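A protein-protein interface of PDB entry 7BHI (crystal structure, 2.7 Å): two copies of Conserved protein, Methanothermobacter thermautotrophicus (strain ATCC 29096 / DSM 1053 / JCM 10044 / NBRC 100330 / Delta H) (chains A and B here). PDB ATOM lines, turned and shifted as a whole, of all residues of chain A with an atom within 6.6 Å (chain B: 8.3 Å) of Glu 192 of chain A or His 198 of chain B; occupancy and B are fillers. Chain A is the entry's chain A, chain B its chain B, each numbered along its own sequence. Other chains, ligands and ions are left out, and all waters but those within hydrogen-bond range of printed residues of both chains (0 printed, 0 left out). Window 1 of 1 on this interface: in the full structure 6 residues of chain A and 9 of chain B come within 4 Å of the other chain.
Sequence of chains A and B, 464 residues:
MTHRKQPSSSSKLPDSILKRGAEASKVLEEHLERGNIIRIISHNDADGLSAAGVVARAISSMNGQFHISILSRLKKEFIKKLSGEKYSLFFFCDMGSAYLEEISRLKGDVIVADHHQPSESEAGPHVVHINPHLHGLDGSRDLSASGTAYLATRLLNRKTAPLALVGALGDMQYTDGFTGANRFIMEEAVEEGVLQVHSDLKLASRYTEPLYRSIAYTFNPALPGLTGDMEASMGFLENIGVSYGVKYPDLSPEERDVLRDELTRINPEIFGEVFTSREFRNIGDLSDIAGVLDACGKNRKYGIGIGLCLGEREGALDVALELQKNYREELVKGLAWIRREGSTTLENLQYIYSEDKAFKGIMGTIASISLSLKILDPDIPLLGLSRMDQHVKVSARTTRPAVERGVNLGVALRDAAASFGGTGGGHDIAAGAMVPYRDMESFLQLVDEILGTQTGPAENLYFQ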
ATOM      1  N   TYR A 150       4.959 -33.823  30.699  1.00  0.00           N
ATOM      2  CA  TYR A 150       4.376 -32.702  29.979  1.00  0.00           C
ATOM      3  C   TYR A 150       4.420 -31.422  30.828  1.00  0.00           C
ATOM      4  O   TYR A 150       4.893 -30.386  30.359  1.00  0.00           O
ATOM      5  CB  TYR A 150       2.958 -33.042  29.519  1.00  0.00           C
ATOM      6  CG  TYR A 150       2.256 -31.955  28.731  1.00  0.00           C
ATOM      7  CD1 TYR A 150       2.759 -31.488  27.523  1.00  0.00           C
ATOM      8  CD2 TYR A 150       1.050 -31.417  29.184  1.00  0.00           C
ATOM      9  CE1 TYR A 150       2.085 -30.511  26.803  1.00  0.00           C
ATOM     10  CE2 TYR A 150       0.370 -30.441  28.469  1.00  0.00           C
ATOM     11  CZ  TYR A 150       0.890 -29.986  27.287  1.00  0.00           C
ATOM     12  OH  TYR A 150       0.200 -28.997  26.614  1.00  0.00           O
ATOM     13  N   ASN A 157       7.228 -26.608  24.866  1.00  0.00           N
ATOM     14  CA  ASN A 157       6.489 -27.242  23.788  1.00  0.00           C
ATOM     15  C   ASN A 157       5.146 -27.720  24.321  1.00  0.00           C
ATOM     16  O   ASN A 157       5.094 -28.485  25.276  1.00  0.00           O
ATOM     17  CB  ASN A 157       7.306 -28.412  23.225  1.00  0.00           C
ATOM     18  CG  ASN A 157       6.759 -28.938  21.907  1.00  0.00           C
ATOM     19  OD1 ASN A 157       5.586 -28.766  21.593  1.00  0.00           O
ATOM     20  ND2 ASN A 157       7.612 -29.569  21.118  1.00  0.00           N
ATOM     21  N   ARG A 158       4.065 -27.248  23.713  1.00  0.00           N
ATOM     22  CA  ARG A 158       2.706 -27.743  23.979  1.00  0.00           C
ATOM     23  C   ARG A 158       2.186 -28.698  22.882  1.00  0.00           C
ATOM     24  O   ARG A 158       1.129 -29.302  23.059  1.00  0.00           O
ATOM     25  CB  ARG A 158       1.742 -26.564  24.130  1.00  0.00           C
ATOM     26  CG  ARG A 158       1.864 -25.790  25.439  1.00  0.00           C
ATOM     27  CD  ARG A 158       1.992 -24.281  25.211  1.00  0.00           C
ATOM     28  NE  ARG A 158       1.284 -23.455  26.195  1.00  0.00           N
ATOM     29  CZ  ARG A 158       1.644 -23.281  27.469  1.00  0.00           C
ATOM     30  NH1 ARG A 158       2.703 -23.903  27.972  1.00  0.00           N
ATOM     31  NH2 ARG A 158       0.928 -22.484  28.260  1.00  0.00           N
ATOM     32  N   LYS A 159       2.907 -28.835  21.764  1.00  0.00           N
ATOM     33  CA  LYS A 159       2.538 -29.783  20.698  1.00  0.00           C
ATOM     34  C   LYS A 159       2.619 -31.259  21.121  1.00  0.00           C
ATOM     35  O   LYS A 159       2.118 -32.136  20.421  1.00  0.00           O
ATOM     36  CB  LYS A 159       3.400 -29.567  19.430  1.00  0.00           C
ATOM     37  CG  LYS A 159       3.257 -28.198  18.772  1.00  0.00           C
ATOM     38  N   ALA A 161       1.163 -32.517  23.812  1.00  0.00           N
ATOM     39  CA  ALA A 161       0.050 -32.788  24.736  1.00  0.00           C
ATOM     40  C   ALA A 161      -0.687 -34.079  24.442  1.00  0.00           C
ATOM     41  O   ALA A 161      -1.085 -34.775  25.375  1.00  0.00           O
ATOM     42  CB  ALA A 161      -0.934 -31.627  24.766  1.00  0.00           C
ATOM     43  N   GLU A 187      -8.033 -30.486  27.619  1.00  0.00           N
ATOM     44  CA  GLU A 187      -8.577 -29.179  27.283  1.00  0.00           C
ATOM     45  C   GLU A 187      -7.491 -28.181  26.878  1.00  0.00           C
ATOM     46  O   GLU A 187      -7.774 -27.246  26.120  1.00  0.00           O
ATOM     47  CB  GLU A 187      -9.382 -28.631  28.455  1.00  0.00           C
ATOM     48  CG  GLU A 187     -10.731 -29.313  28.622  1.00  0.00           C
ATOM     49  CD  GLU A 187     -11.427 -28.984  29.941  1.00  0.00           C
ATOM     50  OE1 GLU A 187     -10.861 -28.235  30.778  1.00  0.00           O
ATOM     51  OE2 GLU A 187     -12.556 -29.482  30.150  1.00  0.00           O
ATOM     52  N   GLU A 188      -6.270 -28.343  27.406  1.00  0.00           N
ATOM     53  CA  GLU A 188      -5.102 -27.562  26.933  1.00  0.00           C
ATOM     54  C   GLU A 188      -4.679 -27.975  25.515  1.00  0.00           C
ATOM     55  O   GLU A 188      -4.368 -27.117  24.699  1.00  0.00           O
ATOM     56  CB  GLU A 188      -3.910 -27.668  27.893  1.00  0.00           C
ATOM     57  CG  GLU A 188      -2.695 -26.836  27.478  1.00  0.00           C
ATOM     58  CD  GLU A 188      -1.697 -26.596  28.599  1.00  0.00           C
ATOM     59  OE1 GLU A 188      -0.514 -26.941  28.408  1.00  0.00           O
ATOM     60  OE2 GLU A 188      -2.079 -26.056  29.657  1.00  0.00           O
ATOM     61  N   ALA A 189      -4.690 -29.276  25.233  1.00  0.00           N
ATOM     62  CA  ALA A 189      -4.487 -29.783  23.868  1.00  0.00           C
ATOM     63  C   ALA A 189      -5.592 -29.339  22.920  1.00  0.00           C
ATOM     64  O   ALA A 189      -5.319 -29.030  21.758  1.00  0.00           O
ATOM     65  CB  ALA A 189      -4.381 -31.305  23.861  1.00  0.00           C
ATOM     66  N   VAL A 190      -6.833 -29.313  23.408  1.00  0.00           N
ATOM     67  CA  VAL A 190      -7.985 -28.935  22.570  1.00  0.00           C
ATOM     68  C   VAL A 190      -7.916 -27.463  22.144  1.00  0.00           C
ATOM     69  O   VAL A 190      -7.952 -27.174  20.953  1.00  0.00           O
ATOM     70  CB  VAL A 190      -9.346 -29.316  23.229  1.00  0.00           C
ATOM     71  CG1 VAL A 190     -10.480 -28.361  22.866  1.00  0.00           C
ATOM     72  CG2 VAL A 190      -9.726 -30.742  22.832  1.00  0.00           C
ATOM     73  N   GLU A 191      -7.805 -26.552  23.107  1.00  0.00           N
ATOM     74  CA  GLU A 191      -7.547 -25.140  22.807  1.00  0.00           C
ATOM     75  C   GLU A 191      -6.406 -24.974  21.755  1.00  0.00           C
ATOM     76  O   GLU A 191      -6.584 -24.236  20.767  1.00  0.00           O
ATOM     77  CB  GLU A 191      -7.246 -24.348  24.086  1.00  0.00           C
ATOM     78  N   GLU A 192      -5.291 -25.705  21.951  1.00  0.00           N
ATOM     79  CA  GLU A 192      -4.080 -25.632  21.079  1.00  0.00           C
ATOM     80  C   GLU A 192      -4.241 -26.251  19.676  1.00  0.00           C
ATOM     81  O   GLU A 192      -3.336 -26.138  18.855  1.00  0.00           O
ATOM     82  CB  GLU A 192      -2.849 -26.288  21.758  1.00  0.00           C
ATOM     83  CG  GLU A 192      -1.922 -25.364  22.542  1.00  0.00           C
ATOM     84  CD  GLU A 192      -0.617 -25.004  21.819  1.00  0.00           C
ATOM     85  OE1 GLU A 192      -0.111 -25.821  20.999  1.00  0.00           O
ATOM     86  OE2 GLU A 192      -0.074 -23.901  22.097  1.00  0.00           O
ATOM     87  N   GLY A 193      -5.362 -26.924  19.417  1.00  0.00           N
ATOM     88  CA  GLY A 193      -5.696 -27.424  18.079  1.00  0.00           C
ATOM     89  C   GLY A 193      -5.031 -28.721  17.642  1.00  0.00           C
ATOM     90  O   GLY A 193      -5.257 -29.180  16.522  1.00  0.00           O
ATOM     91  N   VAL A 194      -4.242 -29.328  18.524  1.00  0.00           N
ATOM     92  CA  VAL A 194      -3.501 -30.565  18.208  1.00  0.00           C
ATOM     93  C   VAL A 194      -4.246 -31.867  18.567  1.00  0.00           C
ATOM     94  O   VAL A 194      -3.756 -32.954  18.276  1.00  0.00           O
ATOM     95  CB  VAL A 194      -2.108 -30.572  18.892  1.00  0.00           C
ATOM     96  CG1 VAL A 194      -1.272 -29.420  18.362  1.00  0.00           C
ATOM     97  CG2 VAL A 194      -2.199 -30.534  20.424  1.00  0.00           C
ATOM     98  N   LEU A 195      -5.401 -31.745  19.228  1.00  0.00           N
ATOM     99  CA  LEU A 195      -6.155 -32.897  19.696  1.00  0.00           C
ATOM    100  C   LEU A 195      -7.633 -32.635  19.465  1.00  0.00           C
ATOM    101  O   LEU A 195      -8.182 -31.699  20.034  1.00  0.00           O
ATOM    102  CB  LEU A 195      -5.875 -33.142  21.186  1.00  0.00           C
ATOM    103  CG  LEU A 195      -6.619 -34.311  21.841  1.00  0.00           C
ATOM    104  CD1 LEU A 195      -6.203 -35.623  21.217  1.00  0.00           C
ATOM    105  CD2 LEU A 195      -6.383 -34.361  23.335  1.00  0.00           C
ATOM    106  N   TYR B 174      -6.860 -19.843   0.848  1.00  0.00           N
ATOM    107  CA  TYR B 174      -6.993 -20.200   2.231  1.00  0.00           C
ATOM    108  C   TYR B 174      -7.995 -19.266   2.927  1.00  0.00           C
ATOM    109  O   TYR B 174      -7.650 -18.158   3.356  1.00  0.00           O
ATOM    110  CB  TYR B 174      -5.621 -20.119   2.866  1.00  0.00           C
ATOM    111  CG  TYR B 174      -5.623 -20.468   4.313  1.00  0.00           C
ATOM    112  CD1 TYR B 174      -5.598 -21.793   4.721  1.00  0.00           C
ATOM    113  CD2 TYR B 174      -5.654 -19.471   5.283  1.00  0.00           C
ATOM    114  CE1 TYR B 174      -5.592 -22.113   6.058  1.00  0.00           C
ATOM    115  CE2 TYR B 174      -5.656 -19.779   6.620  1.00  0.00           C
ATOM    116  CZ  TYR B 174      -5.622 -21.100   7.004  1.00  0.00           C
ATOM    117  OH  TYR B 174      -5.627 -21.387   8.332  1.00  0.00           O
ATOM    118  N   LEU B 195       5.427 -31.577   7.741  1.00  0.00           N
ATOM    119  CA  LEU B 195       4.556 -30.437   7.994  1.00  0.00           C
ATOM    120  C   LEU B 195       3.723 -30.699   9.239  1.00  0.00           C
ATOM    121  O   LEU B 195       2.951 -31.647   9.275  1.00  0.00           O
ATOM    122  CB  LEU B 195       3.650 -30.202   6.792  1.00  0.00           C
ATOM    123  CG  LEU B 195       2.659 -29.041   6.909  1.00  0.00           C
ATOM    124  CD1 LEU B 195       3.379 -27.715   7.024  1.00  0.00           C
ATOM    125  CD2 LEU B 195       1.716 -29.002   5.721  1.00  0.00           C
ATOM    126  N   GLN B 196       3.905 -29.864  10.258  1.00  0.00           N
ATOM    127  CA  GLN B 196       3.147 -29.923  11.501  1.00  0.00           C
ATOM    128  C   GLN B 196       2.064 -28.815  11.567  1.00  0.00           C
ATOM    129  O   GLN B 196       2.170 -27.777  10.896  1.00  0.00           O
ATOM    130  CB  GLN B 196       4.112 -29.828  12.667  1.00  0.00           C
ATOM    131  CG  GLN B 196       5.029 -31.055  12.796  1.00  0.00           C
ATOM    132  CD  GLN B 196       6.218 -31.099  11.812  1.00  0.00           C
ATOM    133  OE1 GLN B 196       6.931 -30.099  11.597  1.00  0.00           O
ATOM    134  NE2 GLN B 196       6.438 -32.275  11.215  1.00  0.00           N
ATOM    135  N   VAL B 197       1.013 -29.072  12.352  1.00  0.00           N
ATOM    136  CA  VAL B 197      -0.146 -28.165  12.513  1.00  0.00           C
ATOM    137  C   VAL B 197      -0.447 -27.904  14.001  1.00  0.00           C
ATOM    138  O   VAL B 197      -0.321 -28.794  14.843  1.00  0.00           O
ATOM    139  CB  VAL B 197      -1.421 -28.732  11.832  1.00  0.00           C
ATOM    140  CG1 VAL B 197      -2.550 -27.717  11.877  1.00  0.00           C
ATOM    141  CG2 VAL B 197      -1.141 -29.122  10.388  1.00  0.00           C
ATOM    142  N   HIS B 198      -0.838 -26.678  14.310  1.00  0.00           N
ATOM    143  CA  HIS B 198      -1.294 -26.318  15.646  1.00  0.00           C
ATOM    144  C   HIS B 198      -2.019 -24.990  15.532  1.00  0.00           C
ATOM    145  O   HIS B 198      -1.667 -24.149  14.708  1.00  0.00           O
ATOM    146  CB  HIS B 198      -0.131 -26.209  16.646  1.00  0.00           C
ATOM    147  CG  HIS B 198       0.896 -25.185  16.279  1.00  0.00           C
ATOM    148  ND1 HIS B 198       1.072 -24.015  16.989  1.00  0.00           N
ATOM    149  CD2 HIS B 198       1.793 -25.148  15.262  1.00  0.00           C
ATOM    150  CE1 HIS B 198       2.038 -23.306  16.433  1.00  0.00           C
ATOM    151  NE2 HIS B 198       2.487 -23.967  15.378  1.00  0.00           N
ATOM    152  N   SER B 199      -3.032 -24.804  16.360  1.00  0.00           N
ATOM    153  CA  SER B 199      -3.795 -23.571  16.378  1.00  0.00           C
ATOM    154  C   SER B 199      -3.090 -22.579  17.298  1.00  0.00           C
ATOM    155  O   SER B 199      -2.751 -22.915  18.429  1.00  0.00           O
ATOM    156  CB  SER B 199      -5.231 -23.860  16.818  1.00  0.00           C
ATOM    157  OG  SER B 199      -5.783 -24.860  15.959  1.00  0.00           O
ATOM    158  N   ASP B 200      -2.849 -21.369  16.803  1.00  0.00           N
ATOM    159  CA  ASP B 200      -2.198 -20.328  17.606  1.00  0.00           C
ATOM    160  C   ASP B 200      -2.610 -18.948  17.071  1.00  0.00           C
ATOM    161  O   ASP B 200      -3.377 -18.855  16.094  1.00  0.00           O
ATOM    162  CB  ASP B 200      -0.672 -20.512  17.544  1.00  0.00           C
ATOM    163  CG  ASP B 200       0.049 -20.167  18.864  1.00  0.00           C
ATOM    164  OD1 ASP B 200      -0.267 -19.132  19.501  1.00  0.00           O
ATOM    165  OD2 ASP B 200       0.959 -20.943  19.239  1.00  0.00           O
ATOM    166  N   LEU B 201      -2.134 -17.885  17.723  1.00  0.00           N
ATOM    167  CA  LEU B 201      -2.246 -16.556  17.157  1.00  0.00           C
ATOM    168  C   LEU B 201      -1.400 -16.501  15.892  1.00  0.00           C
ATOM    169  O   LEU B 201      -0.319 -17.090  15.851  1.00  0.00           O
ATOM    170  CB  LEU B 201      -1.789 -15.494  18.140  1.00  0.00           C
ATOM    171  CG  LEU B 201      -2.593 -15.330  19.440  1.00  0.00           C
ATOM    172  CD1 LEU B 201      -1.972 -14.216  20.287  1.00  0.00           C
ATOM    173  CD2 LEU B 201      -4.071 -15.083  19.153  1.00  0.00           C
ATOM    174  N   LYS B 202      -1.924 -15.843  14.851  1.00  0.00           N
ATOM    175  CA  LYS B 202      -1.284 -15.814  13.534  1.00  0.00           C
ATOM    176  C   LYS B 202      -0.668 -14.445  13.294  1.00  0.00           C
ATOM    177  O   LYS B 202      -0.982 -13.750  12.325  1.00  0.00           O
ATOM    178  CB  LYS B 202      -2.285 -16.181  12.446  1.00  0.00           C
ATOM    179  CG  LYS B 202      -2.742 -17.618  12.502  1.00  0.00           C
ATOM    180  CD  LYS B 202      -4.071 -17.810  11.803  1.00  0.00           C
ATOM    181  CE  LYS B 202      -4.013 -17.311  10.368  1.00  0.00           C
ATOM    182  NZ  LYS B 202      -4.985 -18.011   9.484  1.00  0.00           N
ATOM    183  N   ARG B 206       6.627 -13.989  14.182  1.00  0.00           N
ATOM    184  CA  ARG B 206       6.667 -14.144  15.633  1.00  0.00           C
ATOM    185  C   ARG B 206       8.064 -14.426  16.212  1.00  0.00           C
ATOM    186  O   ARG B 206       8.379 -13.923  17.295  1.00  0.00           O
ATOM    187  CB  ARG B 206       5.637 -15.172  16.118  1.00  0.00           C
ATOM    188  CG  ARG B 206       5.939 -16.637  15.816  1.00  0.00           C
ATOM    189  CD  ARG B 206       4.726 -17.521  16.098  1.00  0.00           C
ATOM    190  NE  ARG B 206       3.551 -17.056  15.352  1.00  0.00           N
ATOM    191  CZ  ARG B 206       2.941 -17.704  14.349  1.00  0.00           C
ATOM    192  NH1 ARG B 206       1.914 -17.125  13.745  1.00  0.00           N
ATOM    193  NH2 ARG B 206       3.313 -18.922  13.939  1.00  0.00           N
ATOM    194  N   TYR B 207       8.910 -15.170  15.490  1.00  0.00           N
ATOM    195  CA  TYR B 207      10.294 -15.435  15.952  1.00  0.00           C
ATOM    196  C   TYR B 207      11.278 -14.267  15.742  1.00  0.00           C
ATOM    197  O   TYR B 207      12.182 -14.115  16.544  1.00  0.00           O
ATOM    198  CB  TYR B 207      10.892 -16.681  15.308  1.00  0.00           C
ATOM    199  CG  TYR B 207       9.996 -17.896  15.298  1.00  0.00           C
ATOM    200  CD1 TYR B 207       9.736 -18.614  16.461  1.00  0.00           C
ATOM    201  CD2 TYR B 207       9.421 -18.334  14.115  1.00  0.00           C
ATOM    202  CE1 TYR B 207       8.904 -19.735  16.444  1.00  0.00           C
ATOM    203  CE2 TYR B 207       8.594 -19.448  14.076  1.00  0.00           C
ATOM    204  CZ  TYR B 207       8.328 -20.152  15.232  1.00  0.00           C
ATOM    205  OH  TYR B 207       7.499 -21.264  15.144  1.00  0.00           O
ATOM    206  N   TYR B 248       7.602 -12.966  20.770  1.00  0.00           N
ATOM    207  CA  TYR B 248       6.362 -13.654  21.192  1.00  0.00           C
ATOM    208  C   TYR B 248       6.573 -14.828  22.134  1.00  0.00           C
ATOM    209  O   TYR B 248       5.907 -14.885  23.161  1.00  0.00           O
ATOM    210  CB  TYR B 248       5.513 -14.049  19.965  1.00  0.00           C
ATOM    211  CG  TYR B 248       4.256 -14.864  20.224  1.00  0.00           C
ATOM    212  CD1 TYR B 248       3.347 -14.502  21.220  1.00  0.00           C
ATOM    213  CD2 TYR B 248       3.948 -15.971  19.430  1.00  0.00           C
ATOM    214  CE1 TYR B 248       2.188 -15.246  21.441  1.00  0.00           C
ATOM    215  CE2 TYR B 248       2.793 -16.719  19.638  1.00  0.00           C
ATOM    216  CZ  TYR B 248       1.915 -16.353  20.640  1.00  0.00           C
ATOM    217  OH  TYR B 248       0.773 -17.080  20.823  1.00  0.00           O
ATOM    218  N   ASP B 257      -1.817 -15.320  27.538  1.00  0.00           N
ATOM    219  CA  ASP B 257      -3.279 -15.505  27.390  1.00  0.00           C
ATOM    220  C   ASP B 257      -4.130 -14.245  27.633  1.00  0.00           C
ATOM    221  O   ASP B 257      -5.318 -14.245  27.313  1.00  0.00           O
ATOM    222  CB  ASP B 257      -3.776 -16.713  28.222  1.00  0.00           C
ATOM    223  CG  ASP B 257      -3.567 -18.048  27.511  1.00  0.00           C
ATOM    224  OD1 ASP B 257      -4.261 -18.296  26.497  1.00  0.00           O
ATOM    225  OD2 ASP B 257      -2.712 -18.849  27.974  1.00  0.00           O
ATOM    226  N   ARG B 260      -4.194 -13.745  23.777  1.00  0.00           N
ATOM    227  CA  ARG B 260      -5.140 -14.568  23.017  1.00  0.00           C
ATOM    228  C   ARG B 260      -6.576 -14.057  23.146  1.00  0.00           C
ATOM    229  O   ARG B 260      -7.265 -13.912  22.146  1.00  0.00           O
ATOM    230  CB  ARG B 260      -5.105 -16.045  23.410  1.00  0.00           C
ATOM    231  CG  ARG B 260      -5.788 -16.938  22.369  1.00  0.00           C
ATOM    232  CD  ARG B 260      -6.399 -18.208  22.950  1.00  0.00           C
ATOM    233  NE  ARG B 260      -7.309 -18.848  21.989  1.00  0.00           N
ATOM    234  CZ  ARG B 260      -7.803 -20.089  22.085  1.00  0.00           C
ATOM    235  NH1 ARG B 260      -7.482 -20.891  23.101  1.00  0.00           N
ATOM    236  NH2 ARG B 260      -8.627 -20.538  21.137  1.00  0.00           N
ATOM    237  N   PHE B 271      -6.995 -16.163  15.718  1.00  0.00           N
ATOM    238  CA  PHE B 271      -6.711 -17.495  16.236  1.00  0.00           C
ATOM    239  C   PHE B 271      -7.137 -18.523  15.218  1.00  0.00           C
ATOM    240  O   PHE B 271      -8.279 -18.505  14.785  1.00  0.00           O
ATOM    241  CB  PHE B 271      -7.427 -17.767  17.560  1.00  0.00           C
ATOM    242  CG  PHE B 271      -6.878 -18.953  18.293  1.00  0.00           C
ATOM    243  CD1 PHE B 271      -5.783 -18.814  19.131  1.00  0.00           C
ATOM    244  CD2 PHE B 271      -7.421 -20.220  18.099  1.00  0.00           C
ATOM    245  CE1 PHE B 271      -5.246 -19.909  19.774  1.00  0.00           C
ATOM    246  CE2 PHE B 271      -6.883 -21.319  18.738  1.00  0.00           C
ATOM    247  CZ  PHE B 271      -5.790 -21.162  19.573  1.00  0.00           C
ATOM    248  N   GLY B 272      -6.230 -19.432  14.857  1.00  0.00           N
ATOM    249  CA  GLY B 272      -6.544 -20.492  13.896  1.00  0.00           C
ATOM    250  C   GLY B 272      -5.346 -21.321  13.497  1.00  0.00           C
ATOM    251  O   GLY B 272      -4.306 -21.257  14.165  1.00  0.00           O
ATOM    252  N   GLU B 273      -5.510 -22.105  12.426  1.00  0.00           N
ATOM    253  CA  GLU B 273      -4.463 -22.988  11.876  1.00  0.00           C
ATOM    254  C   GLU B 273      -3.166 -22.228  11.531  1.00  0.00           C
ATOM    255  O   GLU B 273      -3.179 -21.255  10.761  1.00  0.00           O
ATOM    256  CB  GLU B 273      -4.954 -23.722  10.610  1.00  0.00           C
ATOM    257  CG  GLU B 273      -5.870 -24.930  10.805  1.00  0.00           C
ATOM    258  CD  GLU B 273      -6.354 -25.542   9.474  1.00  0.00           C
ATOM    259  OE1 GLU B 273      -6.585 -26.782   9.408  1.00  0.00           O
ATOM    260  OE2 GLU B 273      -6.518 -24.795   8.482  1.00  0.00           O
ATOM    261  N   VAL B 274      -2.070 -22.690  12.138  1.00  0.00           N
ATOM    262  CA  VAL B 274      -0.700 -22.305  11.828  1.00  0.00           C
ATOM    263  C   VAL B 274       0.000 -23.534  11.213  1.00  0.00           C
ATOM    264  O   VAL B 274      -0.271 -24.677  11.591  1.00  0.00           O
ATOM    265  CB  VAL B 274       0.033 -21.881  13.110  1.00  0.00           C
ATOM    266  CG1 VAL B 274       1.533 -21.780  12.890  1.00  0.00           C
ATOM    267  CG2 VAL B 274      -0.511 -20.558  13.612  1.00  0.00           C
ATOM    268  N   PHE B 275       0.902 -23.291  10.273  1.00  0.00           N
ATOM    269  CA  PHE B 275       1.624 -24.353   9.580  1.00  0.00           C
ATOM    270  C   PHE B 275       3.123 -24.155   9.737  1.00  0.00           C
ATOM    271  O   PHE B 275       3.674 -23.144   9.299  1.00  0.00           O
ATOM    272  CB  PHE B 275       1.261 -24.354   8.111  1.00  0.00           C
ATOM    273  CG  PHE B 275      -0.160 -24.717   7.853  1.00  0.00           C
ATOM    274  CD1 PHE B 275      -1.145 -23.748   7.895  1.00  0.00           C
ATOM    275  CD2 PHE B 275      -0.515 -26.021   7.568  1.00  0.00           C
ATOM    276  CE1 PHE B 275      -2.471 -24.080   7.666  1.00  0.00           C
ATOM    277  CE2 PHE B 275      -1.830 -26.361   7.339  1.00  0.00           C
ATOM    278  CZ  PHE B 275      -2.815 -25.394   7.391  1.00  0.00           C
ATOM    279  N   THR B 276       3.774 -25.110  10.392  1.00  0.00           N
ATOM    280  CA  THR B 276       5.216 -25.084  10.557  1.00  0.00           C
ATOM    281  C   THR B 276       5.832 -26.364   9.959  1.00  0.00           C
ATOM    282  O   THR B 276       5.256 -27.437  10.052  1.00  0.00           O
ATOM    283  CB  THR B 276       5.571 -24.922  12.046  1.00  0.00           C
ATOM    284  OG1 THR B 276       4.961 -25.975  12.799  1.00  0.00           O
ATOM    285  CG2 THR B 276       5.073 -23.567  12.574  1.00  0.00           C
ATOM    286  N   SER B 277       6.978 -26.213   9.307  1.00  0.00           N
ATOM    287  CA  SER B 277       7.777 -27.326   8.793  1.00  0.00           C
ATOM    288  C   SER B 277       9.180 -27.109   9.341  1.00  0.00           C
ATOM    289  O   SER B 277       9.599 -25.972   9.464  1.00  0.00           O
ATOM    290  CB  SER B 277       7.764 -27.317   7.260  1.00  0.00           C
ATOM    291  OG  SER B 277       8.801 -28.120   6.697  1.00  0.00           O
ATOM    292  N   ASP B 285       6.467 -19.619  10.358  1.00  0.00           N
ATOM    293  CA  ASP B 285       5.426 -20.504   9.805  1.00  0.00           C
ATOM    294  C   ASP B 285       5.358 -20.405   8.269  1.00  0.00           C
ATOM    295  O   ASP B 285       5.995 -19.538   7.675  1.00  0.00           O
ATOM    296  CB  ASP B 285       4.054 -20.171  10.416  1.00  0.00           C
ATOM    297  CG  ASP B 285       3.539 -18.775  10.029  1.00  0.00           C
ATOM    298  OD1 ASP B 285       2.963 -18.614   8.930  1.00  0.00           O
ATOM    299  OD2 ASP B 285       3.703 -17.831  10.829  1.00  0.00           O
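1 position is printed for both chains.
Of the 7 pairs that touch across the chains among the printed residues, none has its exchanged pair printed and touching as well.
Of the 22 printed residues of chain B, 5 touch a printed residue of chain A.
Hydrophobic or aromatic side chains of chain A that line the printed part of chain B: Val 194.
Among the printed residues, 7 pairs touch across the chains.
Of chain B, only His 198 (3.8 Å) and Ser 199 (2.8 Å) come within 4 Å of Glu 192 of chain A.
Of the printed residues of chain A, His 198 of chain B touches Glu 192 (3.8 Å) and Val 194 (3.8 Å).
Printed residues of chain B within 4 Å of Gly 193 of chain A: Ser 199 (3.3 Å).
Printed residues of chain A within 4 Å of Phe 271 of chain B: Glu 191 (3.4 Å).
Of the printed residues of chain A, Arg 260 of chain B touches Glu 191.
Of the printed residues of chain A, Val 197 of chain B touches Val 194.
Printed residues of chain B within 4 Å of Val 194 of chain A: Val 197 and His 198.
The nearest residue of chain B that does not touch Glu 192 of chain A is Asp 200 of chain B (4.2 Å).
The nearest printed residue of chain B that does not touch Gly 193 of chain A is His 198 of chain B (4.9 Å).
Among the printed residues, pairs that only touch across the chains: Glu 191 of chain A with Arg 260 of chain B (3.6 Å), Glu 191 of chain A with Phe 271 of chain B (3.4 Å), Glu 192 of chain A with His 198 of chain B (3.8 Å), Gly 193 of chain A with Ser 199 of chain B (3.3 Å), Val 194 of chain A with Val 197 of chain B (3.7 Å) and Val 194 of chain A with His 198 of chain B (3.8 Å).
N of Val 194 of chain A sits at hydrogen-bond distance from O of Ala 189 of chain A, at 3.4 Å.
N of Val 274 of chain B sits at hydrogen-bond distance from O of His 198 of chain B (3.0 Å).
The backbone carbonyl oxygen (O) of Glu 192 of chain A sits at hydrogen-bond distance from the backbone NH (N) of Ser 199 of chain B.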
